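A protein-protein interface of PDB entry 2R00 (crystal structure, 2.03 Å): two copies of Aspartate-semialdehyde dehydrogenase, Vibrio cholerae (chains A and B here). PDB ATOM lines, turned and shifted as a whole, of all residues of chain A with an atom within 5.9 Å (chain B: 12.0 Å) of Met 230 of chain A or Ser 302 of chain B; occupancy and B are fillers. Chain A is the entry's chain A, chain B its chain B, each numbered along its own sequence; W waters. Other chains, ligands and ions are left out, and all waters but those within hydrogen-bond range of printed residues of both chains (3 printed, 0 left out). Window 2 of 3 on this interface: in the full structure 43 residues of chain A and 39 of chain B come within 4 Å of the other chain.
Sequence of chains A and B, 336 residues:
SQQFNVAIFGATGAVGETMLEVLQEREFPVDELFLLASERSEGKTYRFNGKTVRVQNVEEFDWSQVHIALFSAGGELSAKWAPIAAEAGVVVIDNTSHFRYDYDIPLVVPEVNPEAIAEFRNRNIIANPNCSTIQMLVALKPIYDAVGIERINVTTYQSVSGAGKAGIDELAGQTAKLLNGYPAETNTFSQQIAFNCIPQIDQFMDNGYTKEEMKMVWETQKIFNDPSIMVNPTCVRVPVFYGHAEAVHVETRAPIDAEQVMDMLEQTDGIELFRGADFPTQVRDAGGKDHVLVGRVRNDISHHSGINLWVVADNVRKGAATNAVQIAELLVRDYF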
ATOM      1  N   ILE A 149       1.908  -6.049  20.976  1.00  0.00           N
ATOM      2  CA  ILE A 149       3.103  -5.253  21.238  1.00  0.00           C
ATOM      3  C   ILE A 149       3.839  -5.791  22.458  1.00  0.00           C
ATOM      4  O   ILE A 149       3.263  -5.930  23.540  1.00  0.00           O
ATOM      5  CB  ILE A 149       2.789  -3.741  21.427  1.00  0.00           C
ATOM      6  CG1 ILE A 149       2.144  -3.153  20.167  1.00  0.00           C
ATOM      7  CG2 ILE A 149       4.079  -2.968  21.782  1.00  0.00           C
ATOM      8  CD1 ILE A 149       1.658  -1.737  20.327  1.00  0.00           C
ATOM      9  N   GLU A 150       5.117  -6.094  22.255  1.00  0.00           N
ATOM     10  CA  GLU A 150       5.993  -6.624  23.286  1.00  0.00           C
ATOM     11  C   GLU A 150       6.706  -5.478  23.995  1.00  0.00           C
ATOM     12  O   GLU A 150       6.734  -5.416  25.227  1.00  0.00           O
ATOM     13  CB  GLU A 150       7.008  -7.571  22.635  1.00  0.00           C
ATOM     14  CG  GLU A 150       7.886  -8.362  23.586  1.00  0.00           C
ATOM     15  CD  GLU A 150       8.761  -9.376  22.850  1.00  0.00           C
ATOM     16  OE1 GLU A 150       9.116 -10.416  23.460  1.00  0.00           O
ATOM     17  OE2 GLU A 150       9.083  -9.142  21.653  1.00  0.00           O
ATOM     18  N   ARG A 151       7.266  -4.562  23.203  1.00  0.00           N
ATOM     19  CA  ARG A 151       8.045  -3.456  23.730  1.00  0.00           C
ATOM     20  C   ARG A 151       7.843  -2.182  22.906  1.00  0.00           C
ATOM     21  O   ARG A 151       7.828  -2.229  21.674  1.00  0.00           O
ATOM     22  CB  ARG A 151       9.519  -3.843  23.748  1.00  0.00           C
ATOM     23  CG  ARG A 151      10.410  -2.908  24.545  1.00  0.00           C
ATOM     24  CD  ARG A 151      11.873  -3.336  24.468  1.00  0.00           C
ATOM     25  NE  ARG A 151      11.997  -4.778  24.266  1.00  0.00           N
ATOM     26  CZ  ARG A 151      12.568  -5.337  23.202  1.00  0.00           C
ATOM     27  NH1 ARG A 151      13.098  -4.571  22.253  1.00  0.00           N
ATOM     28  NH2 ARG A 151      12.621  -6.661  23.098  1.00  0.00           N
ATOM     29  N   ILE A 152       7.666  -1.057  23.605  1.00  0.00           N
ATOM     30  CA  ILE A 152       7.629   0.276  22.978  1.00  0.00           C
ATOM     31  C   ILE A 152       8.815   1.088  23.485  1.00  0.00           C
ATOM     32  O   ILE A 152       8.999   1.248  24.700  1.00  0.00           O
ATOM     33  CB  ILE A 152       6.329   1.068  23.323  1.00  0.00           C
ATOM     34  CG1 ILE A 152       5.073   0.316  22.862  1.00  0.00           C
ATOM     35  CG2 ILE A 152       6.364   2.475  22.692  1.00  0.00           C
ATOM     36  CD1 ILE A 152       3.779   0.747  23.593  1.00  0.00           C
ATOM     37  N   ASN A 153       9.620   1.586  22.551  1.00  0.00           N
ATOM     38  CA  ASN A 153      10.605   2.613  22.845  1.00  0.00           C
ATOM     39  C   ASN A 153      10.158   3.917  22.178  1.00  0.00           C
ATOM     40  O   ASN A 153       9.918   3.966  20.965  1.00  0.00           O
ATOM     41  CB  ASN A 153      12.001   2.187  22.370  1.00  0.00           C
ATOM     42  CG  ASN A 153      12.633   1.125  23.284  1.00  0.00           C
ATOM     43  OD1 ASN A 153      12.018   0.100  23.574  1.00  0.00           O
ATOM     44  ND2 ASN A 153      13.859   1.376  23.738  1.00  0.00           N
ATOM     45  N   GLN A 221       0.670   1.312  30.188  1.00  0.00           N
ATOM     46  CA  GLN A 221       0.296  -0.011  30.693  1.00  0.00           C
ATOM     47  C   GLN A 221      -1.139  -0.067  31.221  1.00  0.00           C
ATOM     48  O   GLN A 221      -1.828  -1.081  31.039  1.00  0.00           O
ATOM     49  CB  GLN A 221       1.273  -0.449  31.787  1.00  0.00           C
ATOM     50  CG  GLN A 221       2.670  -0.781  31.266  1.00  0.00           C
ATOM     51  CD  GLN A 221       3.645  -1.138  32.374  1.00  0.00           C
ATOM     52  OE1 GLN A 221       3.443  -0.785  33.543  1.00  0.00           O
ATOM     53  NE2 GLN A 221       4.719  -1.826  32.011  1.00  0.00           N
ATOM     54  N   PRO A 227       0.056  -5.240  31.876  1.00  0.00           N
ATOM     55  CA  PRO A 227       1.298  -5.096  32.646  1.00  0.00           C
ATOM     56  C   PRO A 227       2.525  -5.714  31.974  1.00  0.00           C
ATOM     57  O   PRO A 227       3.655  -5.410  32.377  1.00  0.00           O
ATOM     58  CB  PRO A 227       0.988  -5.826  33.962  1.00  0.00           C
ATOM     59  CG  PRO A 227      -0.155  -6.727  33.653  1.00  0.00           C
ATOM     60  CD  PRO A 227      -0.951  -6.039  32.599  1.00  0.00           C
ATOM     61  N   SER A 228       2.307  -6.549  30.956  1.00  0.00           N
ATOM     62  CA  SER A 228       3.401  -7.209  30.234  1.00  0.00           C
ATOM     63  C   SER A 228       4.057  -6.338  29.149  1.00  0.00           C
ATOM     64  O   SER A 228       5.204  -6.591  28.756  1.00  0.00           O
ATOM     65  CB  SER A 228       2.959  -8.561  29.661  1.00  0.00           C
ATOM     66  OG  SER A 228       2.195  -8.415  28.474  1.00  0.00           O
ATOM     67  N   ILE A 229       3.351  -5.314  28.676  1.00  0.00           N
ATOM     68  CA  ILE A 229       3.949  -4.402  27.697  1.00  0.00           C
ATOM     69  C   ILE A 229       5.038  -3.578  28.357  1.00  0.00           C
ATOM     70  O   ILE A 229       4.791  -2.846  29.320  1.00  0.00           O
ATOM     71  CB  ILE A 229       2.949  -3.448  27.030  1.00  0.00           C
ATOM     72  CG1 ILE A 229       1.731  -4.208  26.514  1.00  0.00           C
ATOM     73  CG2 ILE A 229       3.614  -2.742  25.860  1.00  0.00           C
ATOM     74  CD1 ILE A 229       0.703  -3.314  25.819  1.00  0.00           C
ATOM     75  N   MET A 230       6.247  -3.707  27.831  1.00  0.00           N
ATOM     76  CA  MET A 230       7.352  -2.876  28.291  1.00  0.00           C
ATOM     77  C   MET A 230       7.391  -1.567  27.506  1.00  0.00           C
ATOM     78  O   MET A 230       7.198  -1.547  26.288  1.00  0.00           O
ATOM     79  CB  MET A 230       8.673  -3.644  28.222  1.00  0.00           C
ATOM     80  CG  MET A 230       8.734  -4.857  29.191  1.00  0.00           C
ATOM     81  SD  MET A 230       8.679  -4.448  30.970  1.00  0.00           S
ATOM     82  CE  MET A 230       6.949  -4.752  31.369  1.00  0.00           C
ATOM     83  N   VAL A 231       7.606  -0.475  28.232  1.00  0.00           N
ATOM     84  CA  VAL A 231       7.614   0.865  27.663  1.00  0.00           C
ATOM     85  C   VAL A 231       8.887   1.560  28.130  1.00  0.00           C
ATOM     86  O   VAL A 231       9.171   1.623  29.326  1.00  0.00           O
ATOM     87  CB  VAL A 231       6.388   1.695  28.119  1.00  0.00           C
ATOM     88  CG1 VAL A 231       6.328   3.018  27.348  1.00  0.00           C
ATOM     89  CG2 VAL A 231       5.070   0.895  27.951  1.00  0.00           C
ATOM     90  N   ASN A 232       9.651   2.078  27.182  1.00  0.00           N
ATOM     91  CA  ASN A 232      10.926   2.725  27.479  1.00  0.00           C
ATOM     92  C   ASN A 232      10.951   4.138  26.893  1.00  0.00           C
ATOM     93  O   ASN A 232      11.355   4.325  25.742  1.00  0.00           O
ATOM     94  CB  ASN A 232      12.055   1.852  26.923  1.00  0.00           C
ATOM     95  CG  ASN A 232      11.997   0.430  27.467  1.00  0.00           C
ATOM     96  OD1 ASN A 232      12.127   0.226  28.666  1.00  0.00           O
ATOM     97  ND2 ASN A 232      11.761  -0.547  26.595  1.00  0.00           N
ATOM     98  N   ARG B 151      21.472  -5.179  16.835  1.00  0.00           N
ATOM     99  CA  ARG B 151      20.673  -4.161  16.142  1.00  0.00           C
ATOM    100  C   ARG B 151      20.911  -2.772  16.724  1.00  0.00           C
ATOM    101  O   ARG B 151      20.918  -2.590  17.947  1.00  0.00           O
ATOM    102  CB  ARG B 151      19.179  -4.541  16.196  1.00  0.00           C
ATOM    103  CG  ARG B 151      18.200  -3.531  15.552  1.00  0.00           C
ATOM    104  CD  ARG B 151      16.768  -4.084  15.446  1.00  0.00           C
ATOM    105  NE  ARG B 151      16.200  -4.517  16.732  1.00  0.00           N
ATOM    106  CZ  ARG B 151      15.610  -3.716  17.625  1.00  0.00           C
ATOM    107  NH1 ARG B 151      15.503  -2.404  17.413  1.00  0.00           N
ATOM    108  NH2 ARG B 151      15.125  -4.232  18.750  1.00  0.00           N
ATOM    109  N   HIS B 249      19.661   3.450  20.440  1.00  0.00           N
ATOM    110  CA  HIS B 249      19.263   2.235  21.115  1.00  0.00           C
ATOM    111  C   HIS B 249      20.083   1.095  20.521  1.00  0.00           C
ATOM    112  O   HIS B 249      20.236   0.978  19.295  1.00  0.00           O
ATOM    113  CB  HIS B 249      17.767   1.966  20.964  1.00  0.00           C
ATOM    114  CG  HIS B 249      17.328   0.660  21.551  1.00  0.00           C
ATOM    115  ND1 HIS B 249      17.398  -0.528  20.854  1.00  0.00           N
ATOM    116  CD2 HIS B 249      16.843   0.349  22.778  1.00  0.00           C
ATOM    117  CE1 HIS B 249      16.959  -1.513  21.620  1.00  0.00           C
ATOM    118  NE2 HIS B 249      16.616  -1.008  22.792  1.00  0.00           N
ATOM    119  N   VAL B 250      20.614   0.266  21.410  1.00  0.00           N
ATOM    120  CA  VAL B 250      21.431  -0.874  21.038  1.00  0.00           C
ATOM    121  C   VAL B 250      20.804  -2.146  21.590  1.00  0.00           C
ATOM    122  O   VAL B 250      20.453  -2.211  22.776  1.00  0.00           O
ATOM    123  CB  VAL B 250      22.873  -0.721  21.581  1.00  0.00           C
ATOM    124  CG1 VAL B 250      23.724  -1.903  21.173  1.00  0.00           C
ATOM    125  CG2 VAL B 250      23.496   0.562  21.060  1.00  0.00           C
ATOM    126  N   GLU B 251      20.657  -3.139  20.717  1.00  0.00           N
ATOM    127  CA  GLU B 251      20.197  -4.467  21.087  1.00  0.00           C
ATOM    128  C   GLU B 251      21.421  -5.394  21.073  1.00  0.00           C
ATOM    129  O   GLU B 251      21.965  -5.691  20.011  1.00  0.00           O
ATOM    130  CB  GLU B 251      19.137  -4.927  20.088  1.00  0.00           C
ATOM    131  CG  GLU B 251      18.287  -6.102  20.539  1.00  0.00           C
ATOM    132  CD  GLU B 251      17.338  -5.759  21.674  1.00  0.00           C
ATOM    133  OE1 GLU B 251      16.784  -4.638  21.695  1.00  0.00           O
ATOM    134  OE2 GLU B 251      17.148  -6.627  22.548  1.00  0.00           O
ATOM    135  N   THR B 252      21.872  -5.817  22.253  1.00  0.00           N
ATOM    136  CA  THR B 252      23.153  -6.530  22.380  1.00  0.00           C
ATOM    137  C   THR B 252      23.009  -8.041  22.203  1.00  0.00           C
ATOM    138  O   THR B 252      21.895  -8.574  22.220  1.00  0.00           O
ATOM    139  CB  THR B 252      23.890  -6.190  23.712  1.00  0.00           C
ATOM    140  OG1 THR B 252      23.027  -6.421  24.836  1.00  0.00           O
ATOM    141  CG2 THR B 252      24.333  -4.735  23.723  1.00  0.00           C
ATOM    142  N   ALA B 254      24.498 -10.221  24.237  1.00  0.00           N
ATOM    143  CA  ALA B 254      24.340 -10.705  25.608  1.00  0.00           C
ATOM    144  C   ALA B 254      23.955  -9.531  26.508  1.00  0.00           C
ATOM    145  O   ALA B 254      24.394  -8.406  26.268  1.00  0.00           O
ATOM    146  CB  ALA B 254      25.631 -11.350  26.103  1.00  0.00           C
ATOM    147  N   PRO B 255      23.125  -9.778  27.544  1.00  0.00           N
ATOM    148  CA  PRO B 255      22.751  -8.711  28.492  1.00  0.00           C
ATOM    149  C   PRO B 255      23.926  -7.974  29.145  1.00  0.00           C
ATOM    150  O   PRO B 255      24.967  -8.567  29.418  1.00  0.00           O
ATOM    151  CB  PRO B 255      21.914  -9.444  29.555  1.00  0.00           C
ATOM    152  CG  PRO B 255      22.106 -10.910  29.296  1.00  0.00           C
ATOM    153  CD  PRO B 255      22.442 -11.048  27.851  1.00  0.00           C
ATOM    154  N   ILE B 256      23.751  -6.678  29.377  1.00  0.00           N
ATOM    155  CA  ILE B 256      24.762  -5.862  30.041  1.00  0.00           C
ATOM    156  C   ILE B 256      24.080  -4.752  30.834  1.00  0.00           C
ATOM    157  O   ILE B 256      23.089  -4.175  30.379  1.00  0.00           O
ATOM    158  CB  ILE B 256      25.846  -5.308  29.043  1.00  0.00           C
ATOM    159  CG1 ILE B 256      26.997  -4.629  29.804  1.00  0.00           C
ATOM    160  CG2 ILE B 256      25.225  -4.375  27.981  1.00  0.00           C
ATOM    161  CD1 ILE B 256      28.271  -4.416  28.993  1.00  0.00           C
ATOM    162  N   ASP B 257      24.598  -4.473  32.027  1.00  0.00           N
ATOM    163  CA  ASP B 257      24.015  -3.469  32.900  1.00  0.00           C
ATOM    164  C   ASP B 257      24.454  -2.082  32.463  1.00  0.00           C
ATOM    165  O   ASP B 257      25.623  -1.872  32.148  1.00  0.00           O
ATOM    166  CB  ASP B 257      24.432  -3.702  34.354  1.00  0.00           C
ATOM    167  CG  ASP B 257      23.415  -3.170  35.336  1.00  0.00           C
ATOM    168  OD1 ASP B 257      23.568  -2.018  35.795  1.00  0.00           O
ATOM    169  OD2 ASP B 257      22.443  -3.898  35.628  1.00  0.00           O
ATOM    170  N   ALA B 258      23.518  -1.135  32.452  1.00  0.00           N
ATOM    171  CA  ALA B 258      23.829   0.258  32.123  1.00  0.00           C
ATOM    172  C   ALA B 258      24.986   0.808  32.968  1.00  0.00           C
ATOM    173  O   ALA B 258      25.726   1.696  32.524  1.00  0.00           O
ATOM    174  CB  ALA B 258      22.602   1.118  32.286  1.00  0.00           C
ATOM    175  N   ARG B 298      20.860   3.997  29.961  1.00  0.00           N
ATOM    176  CA  ARG B 298      20.008   3.099  30.725  1.00  0.00           C
ATOM    177  C   ARG B 298      19.587   1.893  29.894  1.00  0.00           C
ATOM    178  O   ARG B 298      19.560   1.949  28.652  1.00  0.00           O
ATOM    179  CB  ARG B 298      18.796   3.856  31.306  1.00  0.00           C
ATOM    180  CG  ARG B 298      17.818   4.364  30.286  1.00  0.00           C
ATOM    181  CD  ARG B 298      17.358   5.783  30.594  1.00  0.00           C
ATOM    182  NE  ARG B 298      17.630   6.582  29.409  1.00  0.00           N
ATOM    183  CZ  ARG B 298      16.725   7.072  28.568  1.00  0.00           C
ATOM    184  NH1 ARG B 298      15.426   6.919  28.776  1.00  0.00           N
ATOM    185  NH2 ARG B 298      17.144   7.754  27.514  1.00  0.00           N
ATOM    186  N   ASN B 299      19.301   0.796  30.583  1.00  0.00           N
ATOM    187  CA  ASN B 299      18.742  -0.397  29.959  1.00  0.00           C
ATOM    188  C   ASN B 299      17.280  -0.180  29.610  1.00  0.00           C
ATOM    189  O   ASN B 299      16.617   0.629  30.251  1.00  0.00           O
ATOM    190  CB  ASN B 299      18.825  -1.578  30.921  1.00  0.00           C
ATOM    191  CG  ASN B 299      20.238  -2.038  31.149  1.00  0.00           C
ATOM    192  OD1 ASN B 299      20.785  -1.874  32.238  1.00  0.00           O
ATOM    193  ND2 ASN B 299      20.842  -2.622  30.117  1.00  0.00           N
ATOM    194  N   ASP B 300      16.780  -0.901  28.609  1.00  0.00           N
ATOM    195  CA  ASP B 300      15.341  -1.035  28.453  1.00  0.00           C
ATOM    196  C   ASP B 300      14.859  -1.660  29.750  1.00  0.00           C
ATOM    197  O   ASP B 300      15.542  -2.523  30.302  1.00  0.00           O
ATOM    198  CB  ASP B 300      14.987  -1.970  27.306  1.00  0.00           C
ATOM    199  CG  ASP B 300      15.225  -1.354  25.948  1.00  0.00           C
ATOM    200  OD1 ASP B 300      15.309  -0.108  25.852  1.00  0.00           O
ATOM    201  OD2 ASP B 300      15.341  -2.132  24.981  1.00  0.00           O
ATOM    202  N   ILE B 301      13.697  -1.229  30.233  1.00  0.00           N
ATOM    203  CA  ILE B 301      13.131  -1.772  31.478  1.00  0.00           C
ATOM    204  C   ILE B 301      12.870  -3.284  31.349  1.00  0.00           C
ATOM    205  O   ILE B 301      12.224  -3.737  30.402  1.00  0.00           O
ATOM    206  CB  ILE B 301      11.869  -0.977  31.913  1.00  0.00           C
ATOM    207  CG1 ILE B 301      12.270   0.452  32.288  1.00  0.00           C
ATOM    208  CG2 ILE B 301      11.158  -1.657  33.107  1.00  0.00           C
ATOM    209  CD1 ILE B 301      11.154   1.479  32.202  1.00  0.00           C
ATOM    210  N   SER B 302      13.416  -4.044  32.304  1.00  0.00           N
ATOM    211  CA  SER B 302      13.383  -5.525  32.342  1.00  0.00           C
ATOM    212  C   SER B 302      13.860  -6.204  31.049  1.00  0.00           C
ATOM    213  O   SER B 302      13.365  -7.265  30.663  1.00  0.00           O
ATOM    214  CB  SER B 302      12.006  -6.054  32.797  1.00  0.00           C
ATOM    215  OG  SER B 302      11.226  -6.511  31.698  1.00  0.00           O
ATOM    216  N   HIS B 303      14.839  -5.583  30.397  1.00  0.00           N
ATOM    217  CA  HIS B 303      15.411  -6.084  29.153  1.00  0.00           C
ATOM    218  C   HIS B 303      16.838  -5.560  29.063  1.00  0.00           C
ATOM    219  O   HIS B 303      17.104  -4.538  28.411  1.00  0.00           O
ATOM    220  CB  HIS B 303      14.568  -5.628  27.954  1.00  0.00           C
ATOM    221  CG  HIS B 303      15.085  -6.098  26.631  1.00  0.00           C
ATOM    222  ND1 HIS B 303      15.111  -7.428  26.272  1.00  0.00           N
ATOM    223  CD2 HIS B 303      15.578  -5.412  25.574  1.00  0.00           C
ATOM    224  CE1 HIS B 303      15.610  -7.543  25.054  1.00  0.00           C
ATOM    225  NE2 HIS B 303      15.903  -6.334  24.610  1.00  0.00           N
ATOM    226  N   HIS B 304      17.749  -6.253  29.745  1.00  0.00           N
ATOM    227  CA  HIS B 304      19.131  -5.790  29.877  1.00  0.00           C
ATOM    228  C   HIS B 304      20.021  -6.005  28.642  1.00  0.00           C
ATOM    229  O   HIS B 304      21.165  -5.548  28.613  1.00  0.00           O
ATOM    230  CB  HIS B 304      19.768  -6.361  31.152  1.00  0.00           C
ATOM    231  CG  HIS B 304      19.502  -5.531  32.374  1.00  0.00           C
ATOM    232  ND1 HIS B 304      18.248  -5.051  32.689  1.00  0.00           N
ATOM    233  CD2 HIS B 304      20.330  -5.086  33.349  1.00  0.00           C
ATOM    234  CE1 HIS B 304      18.314  -4.349  33.807  1.00  0.00           C
ATOM    235  NE2 HIS B 304      19.568  -4.351  34.226  1.00  0.00           N
ATOM    236  N   SER B 305      19.505  -6.688  27.626  1.00  0.00           N
ATOM    237  CA  SER B 305      20.204  -6.726  26.343  1.00  0.00           C
ATOM    238  C   SER B 305      19.751  -5.571  25.436  1.00  0.00           C
ATOM    239  O   SER B 305      20.062  -5.533  24.242  1.00  0.00           O
ATOM    240  CB  SER B 305      20.103  -8.101  25.669  1.00  0.00           C
ATOM    241  OG  SER B 305      18.786  -8.408  25.270  1.00  0.00           O
ATOM    242  N   GLY B 306      19.017  -4.630  26.028  1.00  0.00           N
ATOM    243  CA  GLY B 306      18.714  -3.345  25.395  1.00  0.00           C
ATOM    244  C   GLY B 306      19.412  -2.233  26.150  1.00  0.00           C
ATOM    245  O   GLY B 306      19.325  -2.154  27.374  1.00  0.00           O
ATOM    246  N   ILE B 307      20.129  -1.383  25.419  1.00  0.00           N
ATOM    247  CA  ILE B 307      20.816  -0.242  26.008  1.00  0.00           C
ATOM    248  C   ILE B 307      20.456   1.040  25.261  1.00  0.00           C
ATOM    249  O   ILE B 307      20.460   1.081  24.022  1.00  0.00           O
ATOM    250  CB  ILE B 307      22.357  -0.459  26.050  1.00  0.00           C
ATOM    251  CG1 ILE B 307      22.740  -1.456  27.158  1.00  0.00           C
ATOM    252  CG2 ILE B 307      23.116   0.867  26.218  1.00  0.00           C
ATOM    253  CD1 ILE B 307      22.772  -0.844  28.573  1.00  0.00           C
ATOM    254  N   ASN B 308      20.143   2.075  26.033  1.00  0.00           N
ATOM    255  CA  ASN B 308      19.777   3.372  25.496  1.00  0.00           C
ATOM    256  C   ASN B 308      20.802   4.376  25.944  1.00  0.00           C
ATOM    257  O   ASN B 308      21.257   4.312  27.087  1.00  0.00           O
ATOM    258  CB  ASN B 308      18.399   3.798  26.011  1.00  0.00           C
ATOM    259  CG  ASN B 308      17.315   2.807  25.643  1.00  0.00           C
ATOM    260  OD1 ASN B 308      16.893   2.733  24.487  1.00  0.00           O
ATOM    261  ND2 ASN B 308      16.848   2.041  26.631  1.00  0.00           N
HETATM  262  O   HOH W   1      11.943  -3.196  27.684  1.00  0.00           O
HETATM  263  O   HOH W   2      13.637  -2.453  20.794  1.00  0.00           O
HETATM  264  O   HOH W   3      15.069   4.324  22.796  1.00  0.00           O
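N of Ile 301 of chain B sits at hydrogen-bond distance from OD1 of Asn 232 of chain A (2.7 Å). The side-chain sulfur of Met 230 of chain A lies within hydrogen-bond range of the side-chain hydroxyl of Ser 302 of chain B (3.4 Å). OE1 of Glu 251 of chain B lies within salt-bridge range of NH1 of Arg 151 of chain A (3.7 Å). The side-chain amide nitrogen (ND2) of Asn 153 of chain A lies within hydrogen-bond range of the side-chain amide oxygen (OD1) of Asn 308 of chain B, 3.4 Å away. The side-chain sulfur of Met 230 of chain A lies close to the backbone carbonyl oxygen of Ile 301 of chain B (3.7 Å). ND2 of Asn 153 of chain A lies within hydrogen-bond range of OD1 of Asp 300 of chain B.
NH2 of Arg 151 of chain B lies within salt-bridge range of OE1 of Glu 251 of chain B (3.4 Å). The backbone carbonyl oxygen (O) of Arg 298 of chain B sits at hydrogen-bond distance from the backbone NH (N) of Asn 308 of chain B, at 2.7 Å. The backbone NH (N) of Ile 152 of chain A sits at hydrogen-bond distance from the backbone carbonyl oxygen (O) of Met 230 of chain A (2.8 Å). OD1 of Asp 300 of chain B sits at hydrogen-bond distance from ND2 of Asn 308 of chain B (2.8 Å). The backbone NH (N) of Asp 300 of chain B is in hydrogen-bond range of the backbone carbonyl oxygen (O) of Gly 306 of chain B (3.1 Å). OD1 of Asn 153 of chain A lies within hydrogen-bond range of ND2 of Asn 232 of chain A (3.1 Å).
Among the printed residues, merely in contact across the chains: Arg 151 of chain A with Asp 300 of chain B (3.7 Å), Arg 151 of chain A with His 303 of chain B (3.6 Å), Asn 153 of chain A with His 249 of chain B (3.3 Å), Val 231 of chain A with Ile 301 of chain B (3.5 Å) and Asn 232 of chain A with Asp 300 of chain B (3.5 Å).
Of chain B, only Glu 251, Asp 300 and His 303 come within 4 Å of Arg 151 of chain A. No residue of chain B comes within 4 Å of Ile 152 of chain A. No residue of chain B comes within 4 Å of Ile 229 of chain A. Of chain B, only Ile 301 (3.7 Å) and Ser 302 (3.4 Å) come within 4 Å of Met 230 of chain A. Val 231 of chain A touches one residue of chain B. Of the printed residues of chain B, Asn 232 of chain A touches Asp 300 (3.5 Å) and Ile 301 (2.7 Å). Printed residues of chain A within 4 Å of Glu 251 of chain B: Arg 151 (3.7 Å). Printed residues of chain A within 4 Å of Ile 301 of chain B: Met 230, Val 231 and Asn 232. Ser 302 of chain B touches just one residue of chain A: Met 230. The nearest residue of chain B that does not touch Met 230 of chain A is His 303 of chain B (6.0 Å). The nearest residue of chain A that does not touch Ser 302 of chain B is Asn 232 of chain A (5.8 Å). The nearest printed residue of chain B that does not touch Asn 153 of chain A is Ile 307 of chain B (6.6 Å).
Of the 21 printed residues of chain B, 7 touch a printed residue of chain A. Printed residues of chain B that touch a printed residue of chain A: His 249, Glu 251, Asp 300, Ile 301, Ser 302, His 303 and Asn 308. Of the 12 printed residues of chain A, 5 touch a printed residue of chain B. Among the printed residues, Asp or Glu carboxylates within 4 Å of a Lys or Arg side-chain nitrogen of the other chain: Arg 151 of chain A with Glu 251 of chain B.
Position printed for both chains: 151.
Water W2 bridges the guanidinium group of Arg 151 of chain A (2.6 Å) and the guanidinium group of Arg 151 of chain B (3.1 Å). Water W1 bridges O of Ile 301 of chain B (2.8 Å) and ND2 of Asn 232 of chain A (2.9 Å). Water W3 bridges the side-chain amide oxygen of Asn 308 of chain B (3.0 Å) and the side-chain amide nitrogen of Asn 153 of chain A (3.3 Å).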
